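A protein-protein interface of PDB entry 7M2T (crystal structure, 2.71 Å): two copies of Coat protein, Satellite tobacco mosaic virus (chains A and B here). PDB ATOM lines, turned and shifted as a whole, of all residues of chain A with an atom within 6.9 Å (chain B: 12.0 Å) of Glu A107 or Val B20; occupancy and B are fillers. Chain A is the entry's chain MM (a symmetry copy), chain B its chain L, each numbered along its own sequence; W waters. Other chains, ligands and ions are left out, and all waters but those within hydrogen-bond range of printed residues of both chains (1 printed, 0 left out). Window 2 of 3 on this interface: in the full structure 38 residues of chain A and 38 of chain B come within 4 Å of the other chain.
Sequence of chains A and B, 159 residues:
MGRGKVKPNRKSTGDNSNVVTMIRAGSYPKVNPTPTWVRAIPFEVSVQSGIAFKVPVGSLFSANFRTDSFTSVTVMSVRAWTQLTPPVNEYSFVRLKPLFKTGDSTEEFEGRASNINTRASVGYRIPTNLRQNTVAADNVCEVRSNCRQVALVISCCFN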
ATOM      1  N   LEU A  96      -0.668  19.403   2.363  1.00  0.00           N
ATOM      2  CA  LEU A  96      -0.382  20.327   3.453  1.00  0.00           C
ATOM      3  C   LEU A  96       0.818  21.179   3.078  1.00  0.00           C
ATOM      4  O   LEU A  96       1.882  20.642   2.752  1.00  0.00           O
ATOM      5  CB  LEU A  96      -0.112  19.575   4.758  1.00  0.00           C
ATOM      6  CG  LEU A  96      -1.316  18.886   5.392  1.00  0.00           C
ATOM      7  CD1 LEU A  96      -0.910  18.187   6.674  1.00  0.00           C
ATOM      8  CD2 LEU A  96      -2.419  19.892   5.657  1.00  0.00           C
ATOM      9  N   LYS A  97       0.645  22.501   3.131  1.00  0.00           N
ATOM     10  CA  LYS A  97       1.734  23.445   2.908  1.00  0.00           C
ATOM     11  C   LYS A  97       1.996  24.232   4.189  1.00  0.00           C
ATOM     12  O   LYS A  97       1.142  25.034   4.602  1.00  0.00           O
ATOM     13  CB  LYS A  97       1.395  24.394   1.756  1.00  0.00           C
ATOM     14  CG  LYS A  97       2.543  25.298   1.341  1.00  0.00           C
ATOM     15  CD  LYS A  97       2.143  26.256   0.231  1.00  0.00           C
ATOM     16  CE  LYS A  97       1.627  27.570   0.791  1.00  0.00           C
ATOM     17  NZ  LYS A  97       1.233  28.514  -0.293  1.00  0.00           N
ATOM     18  N   PRO A  98       3.138  24.042   4.851  1.00  0.00           N
ATOM     19  CA  PRO A  98       3.360  24.712   6.138  1.00  0.00           C
ATOM     20  C   PRO A  98       3.510  26.213   5.965  1.00  0.00           C
ATOM     21  O   PRO A  98       4.073  26.688   4.976  1.00  0.00           O
ATOM     22  CB  PRO A  98       4.657  24.078   6.653  1.00  0.00           C
ATOM     23  CG  PRO A  98       4.822  22.812   5.860  1.00  0.00           C
ATOM     24  CD  PRO A  98       4.224  23.107   4.520  1.00  0.00           C
ATOM     25  N   PHE A 100       4.559  29.943   8.146  1.00  0.00           N
ATOM     26  CA  PHE A 100       5.320  30.466   9.275  1.00  0.00           C
ATOM     27  C   PHE A 100       5.386  31.981   9.184  1.00  0.00           C
ATOM     28  O   PHE A 100       5.496  32.539   8.088  1.00  0.00           O
ATOM     29  CB  PHE A 100       6.743  29.897   9.320  1.00  0.00           C
ATOM     30  CG  PHE A 100       6.801  28.405   9.466  1.00  0.00           C
ATOM     31  CD1 PHE A 100       6.513  27.804  10.679  1.00  0.00           C
ATOM     32  CD2 PHE A 100       7.160  27.606   8.396  1.00  0.00           C
ATOM     33  CE1 PHE A 100       6.569  26.433  10.818  1.00  0.00           C
ATOM     34  CE2 PHE A 100       7.219  26.235   8.528  1.00  0.00           C
ATOM     35  CZ  PHE A 100       6.922  25.648   9.742  1.00  0.00           C
ATOM     36  N   ASP A 104       6.955  31.688   4.660  1.00  0.00           N
ATOM     37  CA  ASP A 104       6.159  30.521   4.300  1.00  0.00           C
ATOM     38  C   ASP A 104       6.980  29.491   3.533  1.00  0.00           C
ATOM     39  O   ASP A 104       7.943  29.821   2.834  1.00  0.00           O
ATOM     40  CB  ASP A 104       4.949  30.929   3.457  1.00  0.00           C
ATOM     41  CG  ASP A 104       3.877  31.631   4.270  1.00  0.00           C
ATOM     42  OD1 ASP A 104       3.797  31.391   5.495  1.00  0.00           O
ATOM     43  OD2 ASP A 104       3.107  32.419   3.682  1.00  0.00           O
ATOM     44  N   SER A 105       6.575  28.233   3.664  1.00  0.00           N
ATOM     45  CA  SER A 105       7.151  27.128   2.915  1.00  0.00           C
ATOM     46  C   SER A 105       6.430  26.951   1.585  1.00  0.00           C
ATOM     47  O   SER A 105       5.287  27.375   1.409  1.00  0.00           O
ATOM     48  CB  SER A 105       7.071  25.828   3.714  1.00  0.00           C
ATOM     49  OG  SER A 105       8.058  25.783   4.731  1.00  0.00           O
ATOM     50  N   THR A 106       7.115  26.306   0.642  1.00  0.00           N
ATOM     51  CA  THR A 106       6.500  25.911  -0.619  1.00  0.00           C
ATOM     52  C   THR A 106       6.468  24.397  -0.800  1.00  0.00           C
ATOM     53  O   THR A 106       6.196  23.924  -1.910  1.00  0.00           O
ATOM     54  CB  THR A 106       7.213  26.573  -1.804  1.00  0.00           C
ATOM     55  OG1 THR A 106       8.632  26.503  -1.618  1.00  0.00           O
ATOM     56  CG2 THR A 106       6.787  28.026  -1.932  1.00  0.00           C
ATOM     57  N   GLU A 107       6.739  23.628   0.253  1.00  0.00           N
ATOM     58  CA  GLU A 107       6.504  22.192   0.212  1.00  0.00           C
ATOM     59  C   GLU A 107       5.008  21.904   0.143  1.00  0.00           C
ATOM     60  O   GLU A 107       4.186  22.640   0.695  1.00  0.00           O
ATOM     61  CB  GLU A 107       7.096  21.503   1.445  1.00  0.00           C
ATOM     62  CG  GLU A 107       8.605  21.386   1.455  1.00  0.00           C
ATOM     63  CD  GLU A 107       9.294  22.703   1.735  1.00  0.00           C
ATOM     64  OE1 GLU A 107       9.036  23.296   2.804  1.00  0.00           O
ATOM     65  OE2 GLU A 107      10.091  23.146   0.882  1.00  0.00           O
ATOM     66  N   GLU A 108       4.657  20.813  -0.539  1.00  0.00           N
ATOM     67  CA  GLU A 108       3.273  20.356  -0.632  1.00  0.00           C
ATOM     68  C   GLU A 108       3.236  18.862  -0.307  1.00  0.00           C
ATOM     69  O   GLU A 108       3.079  18.028  -1.199  1.00  0.00           O
ATOM     70  CB  GLU A 108       2.684  20.647  -2.014  1.00  0.00           C
ATOM     71  CG  GLU A 108       2.558  22.123  -2.363  1.00  0.00           C
ATOM     72  CD  GLU A 108       1.325  22.774  -1.761  1.00  0.00           C
ATOM     73  OE1 GLU A 108       0.568  22.081  -1.050  1.00  0.00           O
ATOM     74  OE2 GLU A 108       1.108  23.981  -2.005  1.00  0.00           O
ATOM     75  N   PHE A 109       3.394  18.531   0.975  1.00  0.00           N
ATOM     76  CA  PHE A 109       3.288  17.143   1.411  1.00  0.00           C
ATOM     77  C   PHE A 109       1.907  16.596   1.068  1.00  0.00           C
ATOM     78  O   PHE A 109       0.890  17.204   1.408  1.00  0.00           O
ATOM     79  CB  PHE A 109       3.531  17.040   2.918  1.00  0.00           C
ATOM     80  CG  PHE A 109       4.823  17.656   3.376  1.00  0.00           C
ATOM     81  CD1 PHE A 109       6.043  17.089   3.028  1.00  0.00           C
ATOM     82  CD2 PHE A 109       4.821  18.789   4.177  1.00  0.00           C
ATOM     83  CE1 PHE A 109       7.242  17.649   3.460  1.00  0.00           C
ATOM     84  CE2 PHE A 109       6.014  19.357   4.615  1.00  0.00           C
ATOM     85  CZ  PHE A 109       7.227  18.786   4.255  1.00  0.00           C
ATOM     86  N   TYR A 124       3.099  16.671   8.732  1.00  0.00           N
ATOM     87  CA  TYR A 124       4.458  17.186   8.748  1.00  0.00           C
ATOM     88  C   TYR A 124       4.844  17.591  10.162  1.00  0.00           C
ATOM     89  O   TYR A 124       3.997  17.958  10.979  1.00  0.00           O
ATOM     90  CB  TYR A 124       4.639  18.370   7.783  1.00  0.00           C
ATOM     91  CG  TYR A 124       3.946  19.651   8.190  1.00  0.00           C
ATOM     92  CD1 TYR A 124       4.590  20.591   8.985  1.00  0.00           C
ATOM     93  CD2 TYR A 124       2.659  19.933   7.758  1.00  0.00           C
ATOM     94  CE1 TYR A 124       3.965  21.764   9.353  1.00  0.00           C
ATOM     95  CE2 TYR A 124       2.026  21.106   8.120  1.00  0.00           C
ATOM     96  CZ  TYR A 124       2.686  22.016   8.917  1.00  0.00           C
ATOM     97  OH  TYR A 124       2.066  23.186   9.279  1.00  0.00           O
ATOM     98  N   ARG A 125       6.138  17.506  10.438  1.00  0.00           N
ATOM     99  CA  ARG A 125       6.704  17.889  11.719  1.00  0.00           C
ATOM    100  C   ARG A 125       7.377  19.247  11.587  1.00  0.00           C
ATOM    101  O   ARG A 125       7.981  19.556  10.556  1.00  0.00           O
ATOM    102  CB  ARG A 125       7.714  16.842  12.195  1.00  0.00           C
ATOM    103  CG  ARG A 125       8.458  17.202  13.464  1.00  0.00           C
ATOM    104  CD  ARG A 125       9.581  16.210  13.737  1.00  0.00           C
ATOM    105  NE  ARG A 125      10.338  16.545  14.938  1.00  0.00           N
ATOM    106  CZ  ARG A 125      11.441  17.281  14.945  1.00  0.00           C
ATOM    107  NH1 ARG A 125      11.949  17.777  13.828  1.00  0.00           N
ATOM    108  NH2 ARG A 125      12.051  17.525  16.103  1.00  0.00           N
ATOM    109  N   ILE A 126       7.259  20.061  12.622  1.00  0.00           N
ATOM    110  CA  ILE A 126       7.908  21.367  12.682  1.00  0.00           C
ATOM    111  C   ILE A 126       9.214  21.210  13.452  1.00  0.00           C
ATOM    112  O   ILE A 126       9.197  20.654  14.561  1.00  0.00           O
ATOM    113  CB  ILE A 126       6.999  22.415  13.345  1.00  0.00           C
ATOM    114  CG1 ILE A 126       5.697  22.552  12.554  1.00  0.00           C
ATOM    115  CG2 ILE A 126       7.710  23.752  13.450  1.00  0.00           C
ATOM    116  CD1 ILE A 126       4.726  23.547  13.141  1.00  0.00           C
ATOM    117  N   PRO A 127      10.345  21.652  12.911  1.00  0.00           N
ATOM    118  CA  PRO A 127      11.620  21.484  13.617  1.00  0.00           C
ATOM    119  C   PRO A 127      11.751  22.453  14.784  1.00  0.00           C
ATOM    120  O   PRO A 127      11.061  23.472  14.874  1.00  0.00           O
ATOM    121  CB  PRO A 127      12.666  21.775  12.535  1.00  0.00           C
ATOM    122  CG  PRO A 127      11.967  22.716  11.597  1.00  0.00           C
ATOM    123  CD  PRO A 127      10.512  22.311  11.604  1.00  0.00           C
ATOM    124  N   LEU A 130      11.967  26.241  14.609  1.00  0.00           N
ATOM    125  CA  LEU A 130      10.790  26.953  14.127  1.00  0.00           C
ATOM    126  C   LEU A 130       9.601  26.844  15.074  1.00  0.00           C
ATOM    127  O   LEU A 130       8.499  27.272  14.717  1.00  0.00           O
ATOM    128  CB  LEU A 130      10.393  26.446  12.739  1.00  0.00           C
ATOM    129  CG  LEU A 130      11.177  26.986  11.544  1.00  0.00           C
ATOM    130  CD1 LEU A 130      10.754  26.274  10.275  1.00  0.00           C
ATOM    131  CD2 LEU A 130      10.963  28.480  11.400  1.00  0.00           C
ATOM    132  N   ASN B  16      20.463  18.289  14.694  1.00  0.00           N
ATOM    133  CA  ASN B  16      19.065  17.935  14.476  1.00  0.00           C
ATOM    134  C   ASN B  16      18.555  18.530  13.161  1.00  0.00           C
ATOM    135  O   ASN B  16      19.263  19.283  12.491  1.00  0.00           O
ATOM    136  CB  ASN B  16      18.203  18.412  15.648  1.00  0.00           C
ATOM    137  CG  ASN B  16      16.939  17.586  15.820  1.00  0.00           C
ATOM    138  OD1 ASN B  16      16.483  16.923  14.887  1.00  0.00           O
ATOM    139  ND2 ASN B  16      16.366  17.626  17.018  1.00  0.00           N
ATOM    140  N   SER B  17      17.324  18.181  12.796  1.00  0.00           N
ATOM    141  CA  SER B  17      16.732  18.686  11.567  1.00  0.00           C
ATOM    142  C   SER B  17      16.355  20.155  11.709  1.00  0.00           C
ATOM    143  O   SER B  17      15.845  20.587  12.747  1.00  0.00           O
ATOM    144  CB  SER B  17      15.498  17.866  11.203  1.00  0.00           C
ATOM    145  OG  SER B  17      14.837  18.412  10.076  1.00  0.00           O
ATOM    146  N   ASN B  18      16.596  20.923  10.648  1.00  0.00           N
ATOM    147  CA  ASN B  18      16.283  22.345  10.629  1.00  0.00           C
ATOM    148  C   ASN B  18      15.087  22.685   9.756  1.00  0.00           C
ATOM    149  O   ASN B  18      14.754  23.869   9.624  1.00  0.00           O
ATOM    150  CB  ASN B  18      17.496  23.154  10.154  1.00  0.00           C
ATOM    151  CG  ASN B  18      18.612  23.192  11.175  1.00  0.00           C
ATOM    152  OD1 ASN B  18      18.369  23.217  12.384  1.00  0.00           O
ATOM    153  ND2 ASN B  18      19.847  23.201  10.694  1.00  0.00           N
ATOM    154  N   VAL B  19      14.430  21.694   9.154  1.00  0.00           N
ATOM    155  CA  VAL B  19      13.341  21.963   8.227  1.00  0.00           C
ATOM    156  C   VAL B  19      12.143  21.084   8.542  1.00  0.00           C
ATOM    157  O   VAL B  19      12.246  20.063   9.226  1.00  0.00           O
ATOM    158  CB  VAL B  19      13.764  21.763   6.758  1.00  0.00           C
ATOM    159  CG1 VAL B  19      14.656  22.907   6.309  1.00  0.00           C
ATOM    160  CG2 VAL B  19      14.462  20.422   6.589  1.00  0.00           C
ATOM    161  N   VAL B  20      10.988  21.509   8.020  1.00  0.00           N
ATOM    162  CA  VAL B  20       9.782  20.696   8.088  1.00  0.00           C
ATOM    163  C   VAL B  20      10.015  19.380   7.359  1.00  0.00           C
ATOM    164  O   VAL B  20      10.613  19.340   6.276  1.00  0.00           O
ATOM    165  CB  VAL B  20       8.589  21.465   7.491  1.00  0.00           C
ATOM    166  CG1 VAL B  20       8.209  22.630   8.382  1.00  0.00           C
ATOM    167  CG2 VAL B  20       8.928  21.976   6.099  1.00  0.00           C
ATOM    168  N   THR B  21       9.561  18.285   7.962  1.00  0.00           N
ATOM    169  CA  THR B  21       9.714  16.969   7.364  1.00  0.00           C
ATOM    170  C   THR B  21       8.381  16.239   7.376  1.00  0.00           C
ATOM    171  O   THR B  21       7.493  16.530   8.181  1.00  0.00           O
ATOM    172  CB  THR B  21      10.777  16.127   8.086  1.00  0.00           C
ATOM    173  OG1 THR B  21      10.513  16.122   9.495  1.00  0.00           O
ATOM    174  CG2 THR B  21      12.162  16.690   7.828  1.00  0.00           C
ATOM    175  N   MET B  22       8.265  15.269   6.472  1.00  0.00           N
ATOM    176  CA  MET B  22       7.016  14.553   6.270  1.00  0.00           C
ATOM    177  C   MET B  22       6.767  13.532   7.377  1.00  0.00           C
ATOM    178  O   MET B  22       7.696  12.895   7.882  1.00  0.00           O
ATOM    179  CB  MET B  22       7.042  13.856   4.911  1.00  0.00           C
ATOM    180  CG  MET B  22       5.869  12.938   4.644  1.00  0.00           C
ATOM    181  SD  MET B  22       5.081  13.319   3.074  1.00  0.00           S
ATOM    182  CE  MET B  22       6.424  12.994   1.934  1.00  0.00           C
ATOM    183  N   ILE B  23       5.500  13.391   7.759  1.00  0.00           N
ATOM    184  CA  ILE B  23       5.031  12.295   8.597  1.00  0.00           C
ATOM    185  C   ILE B  23       4.197  11.372   7.726  1.00  0.00           C
ATOM    186  O   ILE B  23       3.293  11.830   7.016  1.00  0.00           O
ATOM    187  CB  ILE B  23       4.199  12.798   9.791  1.00  0.00           C
ATOM    188  CG1 ILE B  23       5.074  13.530  10.806  1.00  0.00           C
ATOM    189  CG2 ILE B  23       3.453  11.638  10.446  1.00  0.00           C
ATOM    190  CD1 ILE B  23       4.270  14.227  11.881  1.00  0.00           C
ATOM    191  N   ARG B  24       4.497  10.076   7.775  1.00  0.00           N
ATOM    192  CA  ARG B  24       3.711   9.086   7.042  1.00  0.00           C
ATOM    193  C   ARG B  24       2.603   8.585   7.966  1.00  0.00           C
ATOM    194  O   ARG B  24       2.671   7.506   8.557  1.00  0.00           O
ATOM    195  CB  ARG B  24       4.608   7.965   6.532  1.00  0.00           C
ATOM    196  CG  ARG B  24       5.555   8.443   5.443  1.00  0.00           C
ATOM    197  CD  ARG B  24       6.646   7.445   5.103  1.00  0.00           C
ATOM    198  NE  ARG B  24       7.434   7.913   3.968  1.00  0.00           N
ATOM    199  CZ  ARG B  24       8.399   8.821   4.044  1.00  0.00           C
ATOM    200  NH1 ARG B  24       8.741   9.372   5.198  1.00  0.00           N
ATOM    201  NH2 ARG B  24       9.035   9.188   2.934  1.00  0.00           N
HETATM  202  O   HOH W   1      14.346  19.381  15.355  1.00  0.00           O
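O of Thr B21 sits at hydrogen-bond distance from N of Arg A125 (2.8 Å).
O of Val B19 sits at hydrogen-bond distance from OG of Ser B17 (3.2 Å).
OG of Ser A105 is in hydrogen-bond range of OE1 of Glu A107, at 3.3 Å.
The backbone NH of Phe A100 lies within hydrogen-bond range of the side-chain carboxylate of Asp A104 (3.1 Å).
O of Phe A109 lies within hydrogen-bond range of N of Leu A96, at 2.9 Å.
Among the printed residues, merely in contact across the chains: Tyr A124 with Thr B21, Arg A125 with Val B20, Pro A127 with Ser B17, Pro A127 with Val B19, Glu A107 with Val B20, Phe A100 with Val B20, Pro A127 with Asn B18, Pro A127 with Val B20, Tyr A124 with Ile B23, Phe A109 with Met B22 and Phe A109 with Val B20.
Pro A98 touches none of the printed residues of chain B.
No residue of chain B comes within 4 Å of Thr A106.
No residue of chain B comes within 4 Å of Glu A108.
Of the printed residues of chain B, Phe A109 touches Val B20 and Met B22.
Printed residues of chain B within 4 Å of Pro A127: Ser B17 (3.4 Å), Asn B18 (3.6 Å), Val B19 (3.5 Å) and Val B20 (3.7 Å).
Of the printed residues of chain A, Ser B17 touches Pro A127.
Of the printed residues of chain A, Val B20 touches Phe A100, Glu A107, Phe A109, Arg A125 and Pro A127.
Of the printed residues of chain A, Met B22 touches Phe A109 (3.9 Å).
Of the printed residues of chain A, Ile B23 touches Tyr A124 (3.8 Å).
The nearest residue of chain B that does not touch Glu A107 is Val B19 (6.4 Å).
The nearest printed residue of chain A that does not touch Val B20 is Ser A105 (4.1 Å).
The nearest printed residue of chain B that does not touch Arg A125 is Ile B23 (4.04 Å).
Printed residues of chain B that touch a printed residue of chain A: Ser B17, Asn B18, Val B19, Val B20, Thr B21, Met B22 and Ile B23.
Printed residues of chain A that touch a printed residue of chain B: Phe A100, Glu A107, Phe A109, Tyr A124, Arg A125 and Pro A127.
Hydrophobic or aromatic side chains of chain A within 4 Å of the printed part of chain B: Phe A100, Phe A109, Tyr A124 and Pro A127.
Along chain A the printed residues that touch a printed residue of chain B span positions 100 to 127.
No position is printed for both chains.
Water W1 lies within hydrogen-bond range of NH2 of Arg A125 (3.0 Å), ND2 of Asn B16 (3.2 Å) and O of Ser B17 (3.2 Å).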
